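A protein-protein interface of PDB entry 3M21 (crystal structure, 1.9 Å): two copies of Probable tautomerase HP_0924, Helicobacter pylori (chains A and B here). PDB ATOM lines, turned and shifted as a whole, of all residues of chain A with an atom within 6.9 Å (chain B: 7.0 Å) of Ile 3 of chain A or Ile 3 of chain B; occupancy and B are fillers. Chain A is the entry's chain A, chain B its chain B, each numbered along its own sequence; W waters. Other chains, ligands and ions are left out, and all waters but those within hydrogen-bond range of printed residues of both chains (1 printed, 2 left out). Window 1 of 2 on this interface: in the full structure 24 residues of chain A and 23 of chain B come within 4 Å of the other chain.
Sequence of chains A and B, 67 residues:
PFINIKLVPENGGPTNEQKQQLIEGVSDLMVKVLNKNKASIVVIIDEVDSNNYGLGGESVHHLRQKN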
ATOM      1  N   PRO A   1     -11.657   9.028  29.849  1.00  0.00           N
ATOM      2  CA  PRO A   1     -13.005   9.322  29.300  1.00  0.00           C
ATOM      3  C   PRO A   1     -12.989  10.417  28.227  1.00  0.00           C
ATOM      4  O   PRO A   1     -11.955  11.035  27.974  1.00  0.00           O
ATOM      5  CB  PRO A   1     -13.893   9.722  30.476  1.00  0.00           C
ATOM      6  CG  PRO A   1     -12.867  10.199  31.499  1.00  0.00           C
ATOM      7  CD  PRO A   1     -11.655   9.254  31.306  1.00  0.00           C
ATOM      8  N   PHE A   2     -14.147  10.644  27.610  1.00  0.00           N
ATOM      9  CA  PHE A   2     -14.307  11.644  26.552  1.00  0.00           C
ATOM     10  C   PHE A   2     -15.428  12.599  26.924  1.00  0.00           C
ATOM     11  O   PHE A   2     -16.496  12.176  27.379  1.00  0.00           O
ATOM     12  CB  PHE A   2     -14.646  10.963  25.225  1.00  0.00           C
ATOM     13  CG  PHE A   2     -14.947  11.926  24.106  1.00  0.00           C
ATOM     14  CD1 PHE A   2     -13.943  12.717  23.560  1.00  0.00           C
ATOM     15  CD2 PHE A   2     -16.238  12.038  23.598  1.00  0.00           C
ATOM     16  CE1 PHE A   2     -14.220  13.616  22.516  1.00  0.00           C
ATOM     17  CE2 PHE A   2     -16.528  12.929  22.561  1.00  0.00           C
ATOM     18  CZ  PHE A   2     -15.513  13.718  22.018  1.00  0.00           C
ATOM     19  N   ILE A   3     -15.180  13.891  26.745  1.00  0.00           N
ATOM     20  CA  ILE A   3     -16.180  14.895  27.069  1.00  0.00           C
ATOM     21  C   ILE A   3     -16.271  15.853  25.895  1.00  0.00           C
ATOM     22  O   ILE A   3     -15.254  16.367  25.435  1.00  0.00           O
ATOM     23  CB  ILE A   3     -15.807  15.670  28.347  1.00  0.00           C
ATOM     24  CG1 ILE A   3     -15.663  14.691  29.521  1.00  0.00           C
ATOM     25  CG2 ILE A   3     -16.882  16.688  28.675  1.00  0.00           C
ATOM     26  CD1 ILE A   3     -14.330  13.993  29.572  1.00  0.00           C
ATOM     27  N   ASN A   4     -17.493  16.054  25.398  1.00  0.00           N
ATOM     28  CA  ASN A   4     -17.745  16.939  24.261  1.00  0.00           C
ATOM     29  C   ASN A   4     -18.657  18.046  24.783  1.00  0.00           C
ATOM     30  O   ASN A   4     -19.715  17.783  25.341  1.00  0.00           O
ATOM     31  CB  ASN A   4     -18.421  16.146  23.130  1.00  0.00           C
ATOM     32  CG  ASN A   4     -18.610  16.953  21.858  1.00  0.00           C
ATOM     33  OD1 ASN A   4     -19.507  16.652  21.072  1.00  0.00           O
ATOM     34  ND2 ASN A   4     -17.760  17.970  21.630  1.00  0.00           N
ATOM     35  N   ILE A   5     -18.198  19.285  24.656  1.00  0.00           N
ATOM     36  CA  ILE A   5     -18.962  20.442  25.096  1.00  0.00           C
ATOM     37  C   ILE A   5     -19.305  21.225  23.834  1.00  0.00           C
ATOM     38  O   ILE A   5     -18.423  21.537  23.028  1.00  0.00           O
ATOM     39  CB  ILE A   5     -18.121  21.344  26.043  1.00  0.00           C
ATOM     40  CG1 ILE A   5     -17.592  20.512  27.216  1.00  0.00           C
ATOM     41  CG2 ILE A   5     -18.947  22.511  26.553  1.00  0.00           C
ATOM     42  CD1 ILE A   5     -16.452  21.200  27.998  1.00  0.00           C
ATOM     43  N   LYS A   6     -20.589  21.506  23.643  1.00  0.00           N
ATOM     44  CA  LYS A   6     -21.027  22.272  22.474  1.00  0.00           C
ATOM     45  C   LYS A   6     -21.683  23.532  23.018  1.00  0.00           C
ATOM     46  O   LYS A   6     -22.556  23.447  23.870  1.00  0.00           O
ATOM     47  CB  LYS A   6     -22.046  21.476  21.642  1.00  0.00           C
ATOM     48  CG  LYS A   6     -21.482  20.227  20.975  1.00  0.00           C
ATOM     49  CD  LYS A   6     -22.514  19.531  20.064  1.00  0.00           C
ATOM     50  CE  LYS A   6     -21.927  18.261  19.426  1.00  0.00           C
ATOM     51  NZ  LYS A   6     -20.758  18.559  18.532  1.00  0.00           N
ATOM     52  N   VAL A  26     -13.457  20.263  33.705  1.00  0.00           N
ATOM     53  CA  VAL A  26     -14.113  18.996  33.391  1.00  0.00           C
ATOM     54  C   VAL A  26     -13.195  17.830  33.732  1.00  0.00           C
ATOM     55  O   VAL A  26     -13.640  16.811  34.255  1.00  0.00           O
ATOM     56  CB  VAL A  26     -14.475  18.892  31.889  1.00  0.00           C
ATOM     57  CG1 VAL A  26     -15.077  17.519  31.598  1.00  0.00           C
ATOM     58  CG2 VAL A  26     -15.458  19.988  31.511  1.00  0.00           C
ATOM     59  N   SER A  27     -11.910  17.991  33.435  1.00  0.00           N
ATOM     60  CA  SER A  27     -10.945  16.940  33.706  1.00  0.00           C
ATOM     61  C   SER A  27     -10.789  16.724  35.205  1.00  0.00           C
ATOM     62  O   SER A  27     -10.755  15.584  35.676  1.00  0.00           O
ATOM     63  CB  SER A  27      -9.594  17.284  33.074  1.00  0.00           C
ATOM     64  OG  SER A  27      -9.722  17.412  31.660  1.00  0.00           O
ATOM     65  N   MET A  30     -13.855  14.927  36.626  1.00  0.00           N
ATOM     66  CA  MET A  30     -13.849  13.487  36.391  1.00  0.00           C
ATOM     67  C   MET A  30     -12.933  12.787  37.396  1.00  0.00           C
ATOM     68  O   MET A  30     -13.295  11.756  37.962  1.00  0.00           O
ATOM     69  CB  MET A  30     -13.377  13.170  34.968  1.00  0.00           C
ATOM     70  CG  MET A  30     -14.299  13.669  33.850  1.00  0.00           C
ATOM     71  SD  MET A  30     -15.979  12.990  33.959  1.00  0.00           S
ATOM     72  CE  MET A  30     -16.890  14.458  34.447  1.00  0.00           C
ATOM     73  N   ILE A  41      -8.148  11.684  29.950  1.00  0.00           N
ATOM     74  CA  ILE A  41      -9.336  12.492  29.716  1.00  0.00           C
ATOM     75  C   ILE A  41      -9.192  13.393  28.486  1.00  0.00           C
ATOM     76  O   ILE A  41      -8.307  14.248  28.434  1.00  0.00           O
ATOM     77  CB  ILE A  41      -9.653  13.374  30.940  1.00  0.00           C
ATOM     78  CG1 ILE A  41      -9.913  12.484  32.158  1.00  0.00           C
ATOM     79  CG2 ILE A  41     -10.857  14.261  30.644  1.00  0.00           C
ATOM     80  CD1 ILE A  41     -10.182  13.247  33.431  1.00  0.00           C
ATOM     81  N   VAL A  42     -10.060  13.186  27.498  1.00  0.00           N
ATOM     82  CA  VAL A  42     -10.048  13.989  26.276  1.00  0.00           C
ATOM     83  C   VAL A  42     -11.269  14.892  26.269  1.00  0.00           C
ATOM     84  O   VAL A  42     -12.381  14.454  26.566  1.00  0.00           O
ATOM     85  CB  VAL A  42     -10.077  13.109  25.002  1.00  0.00           C
ATOM     86  CG1 VAL A  42     -10.475  13.954  23.783  1.00  0.00           C
ATOM     87  CG2 VAL A  42      -8.716  12.486  24.770  1.00  0.00           C
ATOM     88  N   VAL A  43     -11.059  16.158  25.928  1.00  0.00           N
ATOM     89  CA  VAL A  43     -12.156  17.103  25.899  1.00  0.00           C
ATOM     90  C   VAL A  43     -12.131  17.845  24.576  1.00  0.00           C
ATOM     91  O   VAL A  43     -11.065  18.186  24.063  1.00  0.00           O
ATOM     92  CB  VAL A  43     -12.051  18.124  27.066  1.00  0.00           C
ATOM     93  CG1 VAL A  43     -13.236  19.083  27.036  1.00  0.00           C
ATOM     94  CG2 VAL A  43     -12.012  17.385  28.402  1.00  0.00           C
ATOM     95  N   ILE A  44     -13.313  18.047  24.005  1.00  0.00           N
ATOM     96  CA  ILE A  44     -13.445  18.783  22.756  1.00  0.00           C
ATOM     97  C   ILE A  44     -14.593  19.766  22.904  1.00  0.00           C
ATOM     98  O   ILE A  44     -15.702  19.406  23.300  1.00  0.00           O
ATOM     99  CB  ILE A  44     -13.712  17.859  21.537  1.00  0.00           C
ATOM    100  CG1 ILE A  44     -12.453  17.049  21.211  1.00  0.00           C
ATOM    101  CG2 ILE A  44     -14.082  18.719  20.313  1.00  0.00           C
ATOM    102  CD1 ILE A  44     -12.617  16.070  20.055  1.00  0.00           C
ATOM    103  N   ILE A  45     -14.306  21.020  22.600  1.00  0.00           N
ATOM    104  CA  ILE A  45     -15.291  22.078  22.698  1.00  0.00           C
ATOM    105  C   ILE A  45     -15.654  22.498  21.279  1.00  0.00           C
ATOM    106  O   ILE A  45     -14.777  22.868  20.489  1.00  0.00           O
ATOM    107  CB  ILE A  45     -14.699  23.296  23.440  1.00  0.00           C
ATOM    108  CG1 ILE A  45     -14.246  22.874  24.835  1.00  0.00           C
ATOM    109  CG2 ILE A  45     -15.721  24.409  23.523  1.00  0.00           C
ATOM    110  CD1 ILE A  45     -13.317  23.853  25.497  1.00  0.00           C
ATOM    111  N   TYR A  53     -28.101  26.712  16.590  1.00  0.00           N
ATOM    112  CA  TYR A  53     -28.440  26.115  17.876  1.00  0.00           C
ATOM    113  C   TYR A  53     -29.874  26.465  18.220  1.00  0.00           C
ATOM    114  O   TYR A  53     -30.254  27.641  18.238  1.00  0.00           O
ATOM    115  CB  TYR A  53     -27.513  26.653  18.970  1.00  0.00           C
ATOM    116  CG  TYR A  53     -27.465  25.851  20.261  1.00  0.00           C
ATOM    117  CD1 TYR A  53     -26.278  25.222  20.672  1.00  0.00           C
ATOM    118  CD2 TYR A  53     -28.586  25.755  21.100  1.00  0.00           C
ATOM    119  CE1 TYR A  53     -26.212  24.523  21.888  1.00  0.00           C
ATOM    120  CE2 TYR A  53     -28.529  25.059  22.311  1.00  0.00           C
ATOM    121  CZ  TYR A  53     -27.338  24.445  22.700  1.00  0.00           C
ATOM    122  OH  TYR A  53     -27.309  23.764  23.906  1.00  0.00           O
ATOM    123  N   PRO B   1     -26.310  25.143  26.399  1.00  0.00           N
ATOM    124  CA  PRO B   1     -25.130  24.329  26.013  1.00  0.00           C
ATOM    125  C   PRO B   1     -25.445  22.841  26.136  1.00  0.00           C
ATOM    126  O   PRO B   1     -26.403  22.451  26.798  1.00  0.00           O
ATOM    127  CB  PRO B   1     -23.995  24.712  26.951  1.00  0.00           C
ATOM    128  CG  PRO B   1     -24.448  26.093  27.430  1.00  0.00           C
ATOM    129  CD  PRO B   1     -25.964  26.009  27.537  1.00  0.00           C
ATOM    130  N   PHE B   2     -24.627  22.026  25.482  1.00  0.00           N
ATOM    131  CA  PHE B   2     -24.783  20.578  25.494  1.00  0.00           C
ATOM    132  C   PHE B   2     -23.447  19.925  25.865  1.00  0.00           C
ATOM    133  O   PHE B   2     -22.419  20.244  25.276  1.00  0.00           O
ATOM    134  CB  PHE B   2     -25.227  20.107  24.106  1.00  0.00           C
ATOM    135  CG  PHE B   2     -25.206  18.618  23.940  1.00  0.00           C
ATOM    136  CD1 PHE B   2     -26.209  17.829  24.489  1.00  0.00           C
ATOM    137  CD2 PHE B   2     -24.154  18.003  23.261  1.00  0.00           C
ATOM    138  CE1 PHE B   2     -26.166  16.436  24.369  1.00  0.00           C
ATOM    139  CE2 PHE B   2     -24.095  16.611  23.133  1.00  0.00           C
ATOM    140  CZ  PHE B   2     -25.108  15.829  23.690  1.00  0.00           C
ATOM    141  N   ILE B   3     -23.462  19.031  26.850  1.00  0.00           N
ATOM    142  CA  ILE B   3     -22.240  18.341  27.269  1.00  0.00           C
ATOM    143  C   ILE B   3     -22.447  16.828  27.248  1.00  0.00           C
ATOM    144  O   ILE B   3     -23.361  16.303  27.887  1.00  0.00           O
ATOM    145  CB  ILE B   3     -21.782  18.733  28.699  1.00  0.00           C
ATOM    146  CG1 ILE B   3     -21.407  20.216  28.766  1.00  0.00           C
ATOM    147  CG2 ILE B   3     -20.572  17.891  29.098  1.00  0.00           C
ATOM    148  CD1 ILE B   3     -22.484  21.089  29.288  1.00  0.00           C
ATOM    149  N   ASN B   4     -21.582  16.139  26.514  1.00  0.00           N
ATOM    150  CA  ASN B   4     -21.657  14.694  26.375  1.00  0.00           C
ATOM    151  C   ASN B   4     -20.456  14.076  27.089  1.00  0.00           C
ATOM    152  O   ASN B   4     -19.313  14.410  26.779  1.00  0.00           O
ATOM    153  CB  ASN B   4     -21.630  14.339  24.885  1.00  0.00           C
ATOM    154  CG  ASN B   4     -21.908  12.875  24.617  1.00  0.00           C
ATOM    155  OD1 ASN B   4     -21.683  12.403  23.505  1.00  0.00           O
ATOM    156  ND2 ASN B   4     -22.418  12.150  25.625  1.00  0.00           N
ATOM    157  N   ILE B   5     -20.717  13.218  28.069  1.00  0.00           N
ATOM    158  CA  ILE B   5     -19.640  12.561  28.803  1.00  0.00           C
ATOM    159  C   ILE B   5     -19.710  11.067  28.512  1.00  0.00           C
ATOM    160  O   ILE B   5     -20.718  10.431  28.793  1.00  0.00           O
ATOM    161  CB  ILE B   5     -19.783  12.738  30.332  1.00  0.00           C
ATOM    162  CG1 ILE B   5     -19.697  14.209  30.710  1.00  0.00           C
ATOM    163  CG2 ILE B   5     -18.695  11.944  31.045  1.00  0.00           C
ATOM    164  CD1 ILE B   5     -20.091  14.481  32.150  1.00  0.00           C
ATOM    165  N   LYS B   6     -18.647  10.518  27.945  1.00  0.00           N
ATOM    166  CA  LYS B   6     -18.606   9.096  27.652  1.00  0.00           C
ATOM    167  C   LYS B   6     -17.512   8.476  28.506  1.00  0.00           C
ATOM    168  O   LYS B   6     -16.365   8.919  28.461  1.00  0.00           O
ATOM    169  CB  LYS B   6     -18.310   8.862  26.173  1.00  0.00           C
ATOM    170  CG  LYS B   6     -19.387   9.397  25.249  1.00  0.00           C
ATOM    171  CD  LYS B   6     -19.131   9.003  23.807  1.00  0.00           C
ATOM    172  CE  LYS B   6     -20.354   9.314  22.965  1.00  0.00           C
ATOM    173  NZ  LYS B   6     -20.142   9.057  21.519  1.00  0.00           N
ATOM    174  N   LEU B  22     -22.004  14.564  38.443  1.00  0.00           N
ATOM    175  CA  LEU B  22     -21.409  14.961  37.172  1.00  0.00           C
ATOM    176  C   LEU B  22     -22.307  15.952  36.455  1.00  0.00           C
ATOM    177  O   LEU B  22     -21.834  16.934  35.886  1.00  0.00           O
ATOM    178  CB  LEU B  22     -21.211  13.743  36.276  1.00  0.00           C
ATOM    179  CG  LEU B  22     -20.176  12.718  36.724  1.00  0.00           C
ATOM    180  CD1 LEU B  22     -20.099  11.612  35.697  1.00  0.00           C
ATOM    181  CD2 LEU B  22     -18.823  13.394  36.899  1.00  0.00           C
ATOM    182  N   VAL B  26     -20.828  19.548  36.042  1.00  0.00           N
ATOM    183  CA  VAL B  26     -20.552  20.093  34.714  1.00  0.00           C
ATOM    184  C   VAL B  26     -21.373  21.345  34.450  1.00  0.00           C
ATOM    185  O   VAL B  26     -20.889  22.311  33.847  1.00  0.00           O
ATOM    186  CB  VAL B  26     -20.869  19.072  33.606  1.00  0.00           C
ATOM    187  CG1 VAL B  26     -20.899  19.766  32.247  1.00  0.00           C
ATOM    188  CG2 VAL B  26     -19.832  17.981  33.616  1.00  0.00           C
ATOM    189  N   SER B  27     -22.620  21.325  34.904  1.00  0.00           N
ATOM    190  CA  SER B  27     -23.513  22.453  34.702  1.00  0.00           C
ATOM    191  C   SER B  27     -23.027  23.685  35.460  1.00  0.00           C
ATOM    192  O   SER B  27     -23.080  24.802  34.940  1.00  0.00           O
ATOM    193  CB  SER B  27     -24.932  22.075  35.132  1.00  0.00           C
ATOM    194  OG  SER B  27     -25.358  20.923  34.430  1.00  0.00           O
ATOM    195  N   MET B  30     -20.010  25.466  33.662  1.00  0.00           N
ATOM    196  CA  MET B  30     -20.430  26.335  32.567  1.00  0.00           C
ATOM    197  C   MET B  30     -20.874  27.693  33.104  1.00  0.00           C
ATOM    198  O   MET B  30     -20.559  28.734  32.524  1.00  0.00           O
ATOM    199  CB  MET B  30     -21.588  25.700  31.794  1.00  0.00           C
ATOM    200  CG  MET B  30     -21.270  24.368  31.133  1.00  0.00           C
ATOM    201  SD  MET B  30     -20.024  24.469  29.848  1.00  0.00           S
ATOM    202  CE  MET B  30     -18.637  23.791  30.715  1.00  0.00           C
ATOM    203  N   ILE B  41     -28.789  24.037  30.273  1.00  0.00           N
ATOM    204  CA  ILE B  41     -27.667  23.115  30.113  1.00  0.00           C
ATOM    205  C   ILE B  41     -28.127  21.654  30.018  1.00  0.00           C
ATOM    206  O   ILE B  41     -28.773  21.149  30.930  1.00  0.00           O
ATOM    207  CB  ILE B  41     -26.660  23.261  31.286  1.00  0.00           C
ATOM    208  CG1 ILE B  41     -26.127  24.702  31.341  1.00  0.00           C
ATOM    209  CG2 ILE B  41     -25.497  22.305  31.103  1.00  0.00           C
ATOM    210  CD1 ILE B  41     -25.149  24.960  32.471  1.00  0.00           C
ATOM    211  N   VAL B  42     -27.824  20.988  28.904  1.00  0.00           N
ATOM    212  CA  VAL B  42     -28.176  19.574  28.747  1.00  0.00           C
ATOM    213  C   VAL B  42     -26.918  18.728  28.910  1.00  0.00           C
ATOM    214  O   VAL B  42     -25.852  19.058  28.384  1.00  0.00           O
ATOM    215  CB  VAL B  42     -28.785  19.257  27.351  1.00  0.00           C
ATOM    216  CG1 VAL B  42     -28.887  17.728  27.154  1.00  0.00           C
ATOM    217  CG2 VAL B  42     -30.158  19.883  27.217  1.00  0.00           C
ATOM    218  N   VAL B  43     -27.050  17.631  29.645  1.00  0.00           N
ATOM    219  CA  VAL B  43     -25.928  16.735  29.866  1.00  0.00           C
ATOM    220  C   VAL B  43     -26.354  15.296  29.590  1.00  0.00           C
ATOM    221  O   VAL B  43     -27.437  14.876  29.981  1.00  0.00           O
ATOM    222  CB  VAL B  43     -25.413  16.823  31.317  1.00  0.00           C
ATOM    223  CG1 VAL B  43     -24.272  15.846  31.521  1.00  0.00           C
ATOM    224  CG2 VAL B  43     -24.936  18.245  31.614  1.00  0.00           C
ATOM    225  N   ILE B  44     -25.500  14.549  28.901  1.00  0.00           N
ATOM    226  CA  ILE B  44     -25.774  13.152  28.603  1.00  0.00           C
ATOM    227  C   ILE B  44     -24.523  12.327  28.898  1.00  0.00           C
ATOM    228  O   ILE B  44     -23.448  12.582  28.348  1.00  0.00           O
ATOM    229  CB  ILE B  44     -26.180  12.940  27.123  1.00  0.00           C
ATOM    230  CG1 ILE B  44     -27.544  13.595  26.855  1.00  0.00           C
ATOM    231  CG2 ILE B  44     -26.280  11.433  26.815  1.00  0.00           C
ATOM    232  CD1 ILE B  44     -28.024  13.414  25.413  1.00  0.00           C
ATOM    233  N   ILE B  45     -24.675  11.351  29.785  1.00  0.00           N
ATOM    234  CA  ILE B  45     -23.575  10.480  30.157  1.00  0.00           C
ATOM    235  C   ILE B  45     -23.786   9.143  29.448  1.00  0.00           C
ATOM    236  O   ILE B  45     -24.833   8.513  29.597  1.00  0.00           O
ATOM    237  CB  ILE B  45     -23.531  10.263  31.706  1.00  0.00           C
ATOM    238  CG1 ILE B  45     -23.429  11.608  32.440  1.00  0.00           C
ATOM    239  CG2 ILE B  45     -22.331   9.398  32.083  1.00  0.00           C
ATOM    240  CD1 ILE B  45     -23.561  11.505  33.963  1.00  0.00           C
ATOM    241  N   TYR B  53     -14.358   0.639  24.133  1.00  0.00           N
ATOM    242  CA  TYR B  53     -13.597   1.864  24.342  1.00  0.00           C
ATOM    243  C   TYR B  53     -12.117   1.583  24.069  1.00  0.00           C
ATOM    244  O   TYR B  53     -11.522   0.677  24.663  1.00  0.00           O
ATOM    245  CB  TYR B  53     -13.798   2.338  25.783  1.00  0.00           C
ATOM    246  CG  TYR B  53     -13.421   3.784  26.038  1.00  0.00           C
ATOM    247  CD1 TYR B  53     -14.396   4.724  26.375  1.00  0.00           C
ATOM    248  CD2 TYR B  53     -12.094   4.209  25.945  1.00  0.00           C
ATOM    249  CE1 TYR B  53     -14.068   6.055  26.617  1.00  0.00           C
ATOM    250  CE2 TYR B  53     -11.741   5.541  26.180  1.00  0.00           C
ATOM    251  CZ  TYR B  53     -12.734   6.458  26.517  1.00  0.00           C
ATOM    252  OH  TYR B  53     -12.391   7.770  26.748  1.00  0.00           O
HETATM  253  O   HOH W   1     -21.148  14.298  21.549  1.00  0.00           O
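N of Lys 6 of chain B sits at hydrogen-bond distance from O of Phe 2 of chain A, at 2.8 Å.
The side-chain hydroxyl (OH) of Tyr 53 of chain B is in hydrogen-bond range of the backbone NH (N) of Phe 2 of chain A (3.5 Å).
The backbone carbonyl oxygen of Asn 4 of chain A lies within hydrogen-bond range of the backbone NH of Asn 4 of chain B, 2.8 Å away.
O of Phe 2 of chain B lies within hydrogen-bond range of N of Lys 6 of chain A, 2.8 Å away.
The backbone carbonyl oxygen (O) of Pro 1 of chain B sits close to the side-chain hydroxyl (OH) of Tyr 53 of chain A (3.3 Å).
The backbone nitrogen (N) of Pro 1 of chain A sits close to the side-chain hydroxyl (OH) of Tyr 53 of chain B, 3.4 Å away.
The backbone NH of Val 42 of chain A is in hydrogen-bond range of the backbone carbonyl oxygen of Pro 1 of chain A, at 2.9 Å.
NZ of Lys 6 of chain A lies close to OD1 of Asn 4 of chain A (3.4 Å).
N of Val 42 of chain B sits at hydrogen-bond distance from O of Pro 1 of chain B (2.9 Å).
O of Ile 3 of chain B lies within hydrogen-bond range of N of Ile 44 of chain B, at 2.9 Å.
ND2 of Asn 4 of chain B lies within hydrogen-bond range of O of Ile 44 of chain B (2.9 Å).
O of Ile 44 of chain B sits at hydrogen-bond distance from N of Ile 5 of chain B, 2.8 Å away.
Among the printed residues, merely in contact across the chains: Pro 1 of chain A with Lys 6 of chain B (3.3 Å), Phe 2 of chain A with Asn 4 of chain B (3.6 Å), Phe 2 of chain A with Ile 5 of chain B (3.5 Å), Ile 3 of chain A with Ile 3 of chain B (3.9 Å), Ile 3 of chain A with Asn 4 of chain B (3.2 Å), Asn 4 of chain A with Phe 2 of chain B (3.7 Å), Asn 4 of chain A with Ile 3 of chain B (3.2 Å), Ile 5 of chain A with Phe 2 of chain B (3.5 Å), Ile 5 of chain A with Met 30 of chain B (3.98 Å), Lys 6 of chain A with Pro 1 of chain B (3.5 Å), Met 30 of chain A with Ile 5 of chain B (3.9 Å), Met 30 of chain A with Leu 22 of chain B (3.3 Å) and Tyr 53 of chain A with Phe 2 of chain B (3.6 Å).
Of the printed residues of chain B, Asn 4 of chain A touches Phe 2, Ile 3 and Asn 4.
Of the printed residues of chain B, Lys 6 of chain A touches Pro 1 and Phe 2.
Val 42 of chain A touches none of the printed residues of chain B.
Val 43 of chain A touches none of the printed residues of chain B.
Printed residues of chain A within 4 Å of Ile 3 of chain B: Ile 3 and Asn 4.
The nearest residue of chain A that does not touch Ile 3 of chain B is Ile 5 of chain A (4.03 Å).
The nearest printed residue of chain A that does not touch Met 30 of chain B is Val 26 of chain A (5.0 Å).
Printed residues of chain B that touch a printed residue of chain A: Pro 1, Phe 2, Ile 3, Asn 4, Ile 5, Lys 6, Leu 22, Met 30 and Tyr 53.
Hydrophobic or aromatic side chains of chain B within 4 Å of the printed part of chain A: Pro 1, Phe 2, Ile 3, Ile 5, Leu 22, Met 30 and Tyr 53.
Of the 15 printed residues of chain A, 8 touch a printed residue of chain B.
Printed residues of chain A that touch a printed residue of chain B: Pro 1, Phe 2, Ile 3, Asn 4, Ile 5, Lys 6, Met 30 and Tyr 53.
Hydrophobic or aromatic side chains of chain A within 4 Å of the printed part of chain B: Pro 1, Ile 3, Ile 5, Met 30 and Tyr 53.
Among the printed residues, 19 pairs touch across the chains.
Among the printed residues, no Asp or Glu carboxylate lies within 4 Å of a Lys or Arg side-chain nitrogen of the other chain.
Pro 1 of chain A touches Lys 6 of chain B, and with the chains exchanged Lys 6 of chain A touches Pro 1 of chain B.
Pro 1 of chain A touches Tyr 53 of chain B, and with the chains exchanged Tyr 53 of chain A touches Pro 1 of chain B.
Phe 2 of chain A touches Ile 5 of chain B, and with the chains exchanged Ile 5 of chain A touches Phe 2 of chain B.
Ile 5 of chain A touches Met 30 of chain B, and with the chains exchanged Met 30 of chain A touches Ile 5 of chain B.
Positions printed for both chains: 1, 2, 3, 4, 5, 6, 26, 27, 30, 41, 42, 43, 44, 45 and 53.
Water W1 lies within hydrogen-bond range of the side-chain amide oxygen (OD1) of Asn 4 of chain B (2.8 Å) and the side-chain amide oxygen (OD1) of Asn 4 of chain A (2.9 Å).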
